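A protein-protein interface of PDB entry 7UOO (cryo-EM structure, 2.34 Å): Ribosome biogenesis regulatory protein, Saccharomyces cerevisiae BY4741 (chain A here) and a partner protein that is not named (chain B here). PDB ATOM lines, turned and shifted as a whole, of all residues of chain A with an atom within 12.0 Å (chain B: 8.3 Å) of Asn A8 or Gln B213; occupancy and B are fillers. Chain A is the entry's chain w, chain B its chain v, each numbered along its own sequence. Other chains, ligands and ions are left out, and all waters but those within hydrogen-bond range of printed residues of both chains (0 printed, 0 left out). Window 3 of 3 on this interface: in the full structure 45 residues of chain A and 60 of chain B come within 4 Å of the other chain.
O of Pro B219 sits at hydrogen-bond distance from NE2 of Gln A59 (3.2 Å).
The guanidinium group of Arg B220 sits close to the backbone carbonyl oxygen of Pro A10 (2.3 Å).
NH1 of Arg B220 lies close to NH1 of Arg A55, at 3.1 Å.
OG of Ser B211 sits at hydrogen-bond distance from O of Leu B218.
The side-chain amide oxygen (OD1) of Asn A63 lies close to the backbone carbonyl oxygen (O) of Gln A59 (2.9 Å).
O of Val A11 is in hydrogen-bond range of ND2 of Asn A63, at 3.3 Å.
The side-chain amide oxygen (OE1) of Gln A59 lies within hydrogen-bond range of the guanidinium group (NH1) of Arg A55 (3.1 Å).
The side-chain hydroxyl of Ser B211 sits at hydrogen-bond distance from the backbone NH of Gly B214 (3.2 Å).
Ser B211 touches Asn A8.
CB of Asn A8 touches CB of Asp B212, 3.8 Å away.
Gln B213 touches Asn A8.
O of Leu A9 touches O of Ser B211 (3.8 Å).
Arg B220 touches Leu A9 (NH2 to CD1, 3.4 Å).
CA of Pro A10 touches OE1 of Gln B213, at 3.9 Å.
CG1 of Val A11 touches CB of Ser B211, at 3.7 Å.
O of Leu B218 touches CG1 of Val A11, 3.98 Å away.
CG1 of Val A11 touches CA of Arg B220, at 3.9 Å.
Asn A8 touches just these residues of chain B: Ser B211, Asp B212 and Gln B213.
Printed residues of chain A within 4 Å of Gln B213: Asn A8 and Pro A10.
Of chain A, only Asn A8 (3.6 Å), Leu A9 (3.8 Å) and Val A11 (3.7 Å) come within 4 Å of Ser B211.
Asp B212 touches one residue of chain A.
Of the printed residues of chain B, Gln A59 touches Pro B219 (3.2 Å).
Printed residues of chain A within 4 Å of Leu B218: Val A11 (3.98 Å).
Of the printed residues of chain B, Pro A10 touches Gln B213 and Arg B220.
Printed residues of chain B within 4 Å of Arg A55: Arg B220 (3.1 Å).
Asn A63 touches none of the printed residues of chain B.
The nearest residue of chain B that does not touch Asn A8 is Lys B210 (5.4 Å).
The nearest printed residue of chain B that does not touch Pro A10 is Ser B211 (5.9 Å).
Of the 10 printed residues of chain A, 6 touch a printed residue of chain B.
Hydrophobic or aromatic side chains of chain A within 4 Å of the printed part of chain B: Leu A9 and Val A11.
Among the printed residues, 12 pairs touch across the chains.
Among the printed residues, no Asp or Glu carboxylate lies within 4 Å of a Lys or Arg side-chain nitrogen of the other chain.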
ATOM      1  N   ASN A   8       5.518  16.920 -24.569  1.00  0.00           N
ATOM      2  CA  ASN A   8       4.679  17.280 -25.707  1.00  0.00           C
ATOM      3  C   ASN A   8       3.262  16.739 -25.534  1.00  0.00           C
ATOM      4  O   ASN A   8       2.888  15.727 -26.128  1.00  0.00           O
ATOM      5  CB  ASN A   8       5.298  16.768 -27.010  1.00  0.00           C
ATOM      6  CG  ASN A   8       5.814  15.347 -26.893  1.00  0.00           C
ATOM      7  OD1 ASN A   8       6.908  15.112 -26.383  1.00  0.00           O
ATOM      8  ND2 ASN A   8       5.026  14.391 -27.371  1.00  0.00           N
ATOM      9  N   LEU A   9       2.481  17.427 -24.707  1.00  0.00           N
ATOM     10  CA  LEU A   9       1.108  17.029 -24.453  1.00  0.00           C
ATOM     11  C   LEU A   9       0.230  17.326 -25.670  1.00  0.00           C
ATOM     12  O   LEU A   9       0.517  18.243 -26.444  1.00  0.00           O
ATOM     13  CB  LEU A   9       0.571  17.757 -23.224  1.00  0.00           C
ATOM     14  CG  LEU A   9       1.311  17.465 -21.919  1.00  0.00           C
ATOM     15  CD1 LEU A   9       0.810  18.358 -20.795  1.00  0.00           C
ATOM     16  CD2 LEU A   9       1.168  15.998 -21.548  1.00  0.00           C
ATOM     17  N   PRO A  10      -0.841  16.557 -25.868  1.00  0.00           N
ATOM     18  CA  PRO A  10      -1.724  16.803 -27.014  1.00  0.00           C
ATOM     19  C   PRO A  10      -2.528  18.082 -26.844  1.00  0.00           C
ATOM     20  O   PRO A  10      -2.751  18.576 -25.738  1.00  0.00           O
ATOM     21  CB  PRO A  10      -2.645  15.575 -27.029  1.00  0.00           C
ATOM     22  CG  PRO A  10      -1.984  14.567 -26.142  1.00  0.00           C
ATOM     23  CD  PRO A  10      -1.241  15.355 -25.119  1.00  0.00           C
ATOM     24  N   VAL A  11      -2.965  18.624 -27.979  1.00  0.00           N
ATOM     25  CA  VAL A  11      -3.811  19.809 -28.006  1.00  0.00           C
ATOM     26  C   VAL A  11      -5.161  19.515 -28.659  1.00  0.00           C
ATOM     27  O   VAL A  11      -5.877  20.430 -29.046  1.00  0.00           O
ATOM     28  CB  VAL A  11      -3.101  20.986 -28.701  1.00  0.00           C
ATOM     29  CG1 VAL A  11      -1.851  21.378 -27.931  1.00  0.00           C
ATOM     30  CG2 VAL A  11      -2.758  20.633 -30.140  1.00  0.00           C
ATOM     31  N   THR A  12      -5.516  18.239 -28.777  1.00  0.00           N
ATOM     32  CA  THR A  12      -6.777  17.811 -29.379  1.00  0.00           C
ATOM     33  C   THR A  12      -7.651  17.221 -28.276  1.00  0.00           C
ATOM     34  O   THR A  12      -7.615  16.019 -28.011  1.00  0.00           O
ATOM     35  CB  THR A  12      -6.540  16.796 -30.492  1.00  0.00           C
ATOM     36  OG1 THR A  12      -6.084  15.562 -29.924  1.00  0.00           O
ATOM     37  CG2 THR A  12      -5.493  17.307 -31.457  1.00  0.00           C
ATOM     38  N   VAL A  13      -8.444  18.074 -27.638  1.00  0.00           N
ATOM     39  CA  VAL A  13      -9.357  17.627 -26.592  1.00  0.00           C
ATOM     40  C   VAL A  13     -10.562  16.963 -27.247  1.00  0.00           C
ATOM     41  O   VAL A  13     -11.247  17.572 -28.074  1.00  0.00           O
ATOM     42  CB  VAL A  13      -9.793  18.795 -25.697  1.00  0.00           C
ATOM     43  CG1 VAL A  13     -10.958  18.377 -24.820  1.00  0.00           C
ATOM     44  CG2 VAL A  13      -8.627  19.272 -24.847  1.00  0.00           C
ATOM     45  N   GLU A  14     -10.819  15.712 -26.878  1.00  0.00           N
ATOM     46  CA  GLU A  14     -11.974  14.973 -27.364  1.00  0.00           C
ATOM     47  C   GLU A  14     -13.060  14.960 -26.298  1.00  0.00           C
ATOM     48  O   GLU A  14     -12.794  14.664 -25.130  1.00  0.00           O
ATOM     49  CB  GLU A  14     -11.593  13.539 -27.738  1.00  0.00           C
ATOM     50  CG  GLU A  14     -10.543  13.436 -28.829  1.00  0.00           C
ATOM     51  CD  GLU A  14     -10.277  12.000 -29.234  1.00  0.00           C
ATOM     52  OE1 GLU A  14     -10.927  11.096 -28.668  1.00  0.00           O
ATOM     53  OE2 GLU A  14      -9.421  11.773 -30.114  1.00  0.00           O
ATOM     54  N   ARG A  55      -9.381  23.294 -18.068  1.00  0.00           N
ATOM     55  CA  ARG A  55      -8.250  23.294 -18.987  1.00  0.00           C
ATOM     56  C   ARG A  55      -8.659  22.788 -20.362  1.00  0.00           C
ATOM     57  O   ARG A  55      -8.283  23.377 -21.383  1.00  0.00           O
ATOM     58  CB  ARG A  55      -7.122  22.437 -18.405  1.00  0.00           C
ATOM     59  CG  ARG A  55      -5.710  22.893 -18.740  1.00  0.00           C
ATOM     60  CD  ARG A  55      -5.322  22.535 -20.158  1.00  0.00           C
ATOM     61  NE  ARG A  55      -5.622  21.145 -20.475  1.00  0.00           N
ATOM     62  CZ  ARG A  55      -5.442  20.596 -21.668  1.00  0.00           C
ATOM     63  NH1 ARG A  55      -4.959  21.292 -22.684  1.00  0.00           N
ATOM     64  NH2 ARG A  55      -5.755  19.316 -21.846  1.00  0.00           N
ATOM     65  N   GLN A  59      -8.715  24.997 -23.750  1.00  0.00           N
ATOM     66  CA  GLN A  59      -7.985  24.567 -24.938  1.00  0.00           C
ATOM     67  C   GLN A  59      -8.873  24.606 -26.174  1.00  0.00           C
ATOM     68  O   GLN A  59      -8.451  25.085 -27.235  1.00  0.00           O
ATOM     69  CB  GLN A  59      -7.421  23.163 -24.730  1.00  0.00           C
ATOM     70  CG  GLN A  59      -6.539  22.677 -25.867  1.00  0.00           C
ATOM     71  CD  GLN A  59      -5.180  23.346 -25.878  1.00  0.00           C
ATOM     72  OE1 GLN A  59      -4.490  23.387 -24.860  1.00  0.00           O
ATOM     73  NE2 GLN A  59      -4.790  23.879 -27.027  1.00  0.00           N
ATOM     74  N   ASN A  63      -8.360  27.115 -29.363  1.00  0.00           N
ATOM     75  CA  ASN A  63      -8.300  26.590 -30.725  1.00  0.00           C
ATOM     76  C   ASN A  63      -9.245  27.351 -31.646  1.00  0.00           C
ATOM     77  O   ASN A  63      -8.860  27.768 -32.747  1.00  0.00           O
ATOM     78  CB  ASN A  63      -8.636  25.097 -30.727  1.00  0.00           C
ATOM     79  CG  ASN A  63      -7.563  24.252 -30.067  1.00  0.00           C
ATOM     80  OD1 ASN A  63      -6.626  24.773 -29.465  1.00  0.00           O
ATOM     81  ND2 ASN A  63      -7.702  22.936 -30.172  1.00  0.00           N
ATOM     82  N   LYS B 210       4.901  25.450 -26.025  1.00  0.00           N
ATOM     83  CA  LYS B 210       5.030  24.800 -27.321  1.00  0.00           C
ATOM     84  C   LYS B 210       4.470  23.385 -27.248  1.00  0.00           C
ATOM     85  O   LYS B 210       4.658  22.676 -26.256  1.00  0.00           O
ATOM     86  CB  LYS B 210       6.491  24.772 -27.763  1.00  0.00           C
ATOM     87  CG  LYS B 210       6.678  24.503 -29.246  1.00  0.00           C
ATOM     88  CD  LYS B 210       6.407  25.752 -30.069  1.00  0.00           C
ATOM     89  CE  LYS B 210       6.130  25.411 -31.523  1.00  0.00           C
ATOM     90  NZ  LYS B 210       7.127  24.457 -32.077  1.00  0.00           N
ATOM     91  N   SER B 211       3.777  22.973 -28.307  1.00  0.00           N
ATOM     92  CA  SER B 211       3.011  21.734 -28.285  1.00  0.00           C
ATOM     93  C   SER B 211       3.701  20.566 -28.973  1.00  0.00           C
ATOM     94  O   SER B 211       3.492  19.420 -28.561  1.00  0.00           O
ATOM     95  CB  SER B 211       1.641  21.952 -28.934  1.00  0.00           C
ATOM     96  OG  SER B 211       1.773  22.429 -30.261  1.00  0.00           O
ATOM     97  N   ASP B 212       4.475  20.820 -30.030  1.00  0.00           N
ATOM     98  CA  ASP B 212       5.196  19.837 -30.841  1.00  0.00           C
ATOM     99  C   ASP B 212       4.259  18.905 -31.607  1.00  0.00           C
ATOM    100  O   ASP B 212       4.736  18.039 -32.349  1.00  0.00           O
ATOM    101  CB  ASP B 212       6.185  18.997 -30.014  1.00  0.00           C
ATOM    102  CG  ASP B 212       7.337  18.462 -30.843  1.00  0.00           C
ATOM    103  OD1 ASP B 212       7.451  18.845 -32.025  1.00  0.00           O
ATOM    104  OD2 ASP B 212       8.127  17.654 -30.311  1.00  0.00           O
ATOM    105  N   GLN B 213       2.943  19.055 -31.462  1.00  0.00           N
ATOM    106  CA  GLN B 213       1.976  18.280 -32.223  1.00  0.00           C
ATOM    107  C   GLN B 213       0.884  19.134 -32.847  1.00  0.00           C
ATOM    108  O   GLN B 213       0.076  18.600 -33.616  1.00  0.00           O
ATOM    109  CB  GLN B 213       1.324  17.203 -31.341  1.00  0.00           C
ATOM    110  CG  GLN B 213       2.260  16.069 -30.948  1.00  0.00           C
ATOM    111  CD  GLN B 213       1.551  14.955 -30.200  1.00  0.00           C
ATOM    112  OE1 GLN B 213       0.393  15.094 -29.803  1.00  0.00           O
ATOM    113  NE2 GLN B 213       2.245  13.838 -30.007  1.00  0.00           N
ATOM    114  N   GLY B 214       0.823  20.424 -32.534  1.00  0.00           N
ATOM    115  CA  GLY B 214      -0.111  21.326 -33.174  1.00  0.00           C
ATOM    116  C   GLY B 214       0.599  22.368 -34.011  1.00  0.00           C
ATOM    117  O   GLY B 214       0.032  23.420 -34.322  1.00  0.00           O
ATOM    118  N   GLY B 215       1.847  22.084 -34.380  1.00  0.00           N
ATOM    119  CA  GLY B 215       2.628  23.035 -35.142  1.00  0.00           C
ATOM    120  C   GLY B 215       3.035  24.233 -34.300  1.00  0.00           C
ATOM    121  O   GLY B 215       3.178  24.156 -33.078  1.00  0.00           O
ATOM    122  N   LYS B 216       3.231  25.362 -34.976  1.00  0.00           N
ATOM    123  CA  LYS B 216       3.564  26.617 -34.319  1.00  0.00           C
ATOM    124  C   LYS B 216       2.364  27.542 -34.195  1.00  0.00           C
ATOM    125  O   LYS B 216       2.534  28.724 -33.879  1.00  0.00           O
ATOM    126  CB  LYS B 216       4.699  27.318 -35.067  1.00  0.00           C
ATOM    127  CG  LYS B 216       4.384  27.641 -36.519  1.00  0.00           C
ATOM    128  CD  LYS B 216       5.641  28.039 -37.280  1.00  0.00           C
ATOM    129  CE  LYS B 216       6.306  29.263 -36.670  1.00  0.00           C
ATOM    130  NZ  LYS B 216       5.444  30.472 -36.759  1.00  0.00           N
ATOM    131  N   ARG B 217       1.156  27.035 -34.436  1.00  0.00           N
ATOM    132  CA  ARG B 217      -0.054  27.844 -34.391  1.00  0.00           C
ATOM    133  C   ARG B 217      -0.936  27.568 -33.184  1.00  0.00           C
ATOM    134  O   ARG B 217      -1.635  28.477 -32.733  1.00  0.00           O
ATOM    135  CB  ARG B 217      -0.885  27.629 -35.663  1.00  0.00           C
ATOM    136  CG  ARG B 217      -0.074  27.611 -36.949  1.00  0.00           C
ATOM    137  CD  ARG B 217       0.666  28.920 -37.176  1.00  0.00           C
ATOM    138  NE  ARG B 217      -0.232  30.068 -37.199  1.00  0.00           N
ATOM    139  CZ  ARG B 217      -0.953  30.435 -38.250  1.00  0.00           C
ATOM    140  NH1 ARG B 217      -0.923  29.752 -39.382  1.00  0.00           N
ATOM    141  NH2 ARG B 217      -1.727  31.513 -38.161  1.00  0.00           N
ATOM    142  N   LEU B 218      -0.919  26.347 -32.647  1.00  0.00           N
ATOM    143  CA  LEU B 218      -1.808  25.938 -31.559  1.00  0.00           C
ATOM    144  C   LEU B 218      -0.976  25.533 -30.349  1.00  0.00           C
ATOM    145  O   LEU B 218      -0.567  24.368 -30.227  1.00  0.00           O
ATOM    146  CB  LEU B 218      -2.714  24.791 -31.999  1.00  0.00           C
ATOM    147  CG  LEU B 218      -3.528  25.020 -33.271  1.00  0.00           C
ATOM    148  CD1 LEU B 218      -4.335  23.781 -33.603  1.00  0.00           C
ATOM    149  CD2 LEU B 218      -4.435  26.232 -33.120  1.00  0.00           C
ATOM    150  N   PRO B 219      -0.711  26.454 -29.430  1.00  0.00           N
ATOM    151  CA  PRO B 219       0.090  26.118 -28.251  1.00  0.00           C
ATOM    152  C   PRO B 219      -0.700  25.312 -27.231  1.00  0.00           C
ATOM    153  O   PRO B 219      -1.930  25.334 -27.186  1.00  0.00           O
ATOM    154  CB  PRO B 219       0.466  27.492 -27.687  1.00  0.00           C
ATOM    155  CG  PRO B 219      -0.675  28.357 -28.079  1.00  0.00           C
ATOM    156  CD  PRO B 219      -1.135  27.864 -29.425  1.00  0.00           C
ATOM    157  N   ARG B 220       0.047  24.586 -26.402  1.00  0.00           N
ATOM    158  CA  ARG B 220      -0.534  23.878 -25.271  1.00  0.00           C
ATOM    159  C   ARG B 220      -0.841  24.866 -24.154  1.00  0.00           C
ATOM    160  O   ARG B 220      -0.006  25.708 -23.810  1.00  0.00           O
ATOM    161  CB  ARG B 220       0.421  22.793 -24.777  1.00  0.00           C
ATOM    162  CG  ARG B 220      -0.003  22.115 -23.483  1.00  0.00           C
ATOM    163  CD  ARG B 220      -1.175  21.169 -23.689  1.00  0.00           C
ATOM    164  NE  ARG B 220      -1.484  20.433 -22.470  1.00  0.00           N
ATOM    165  CZ  ARG B 220      -2.354  19.435 -22.393  1.00  0.00           C
ATOM    166  NH1 ARG B 220      -3.021  19.016 -23.455  1.00  0.00           N
ATOM    167  NH2 ARG B 220      -2.557  18.842 -21.221  1.00  0.00           N
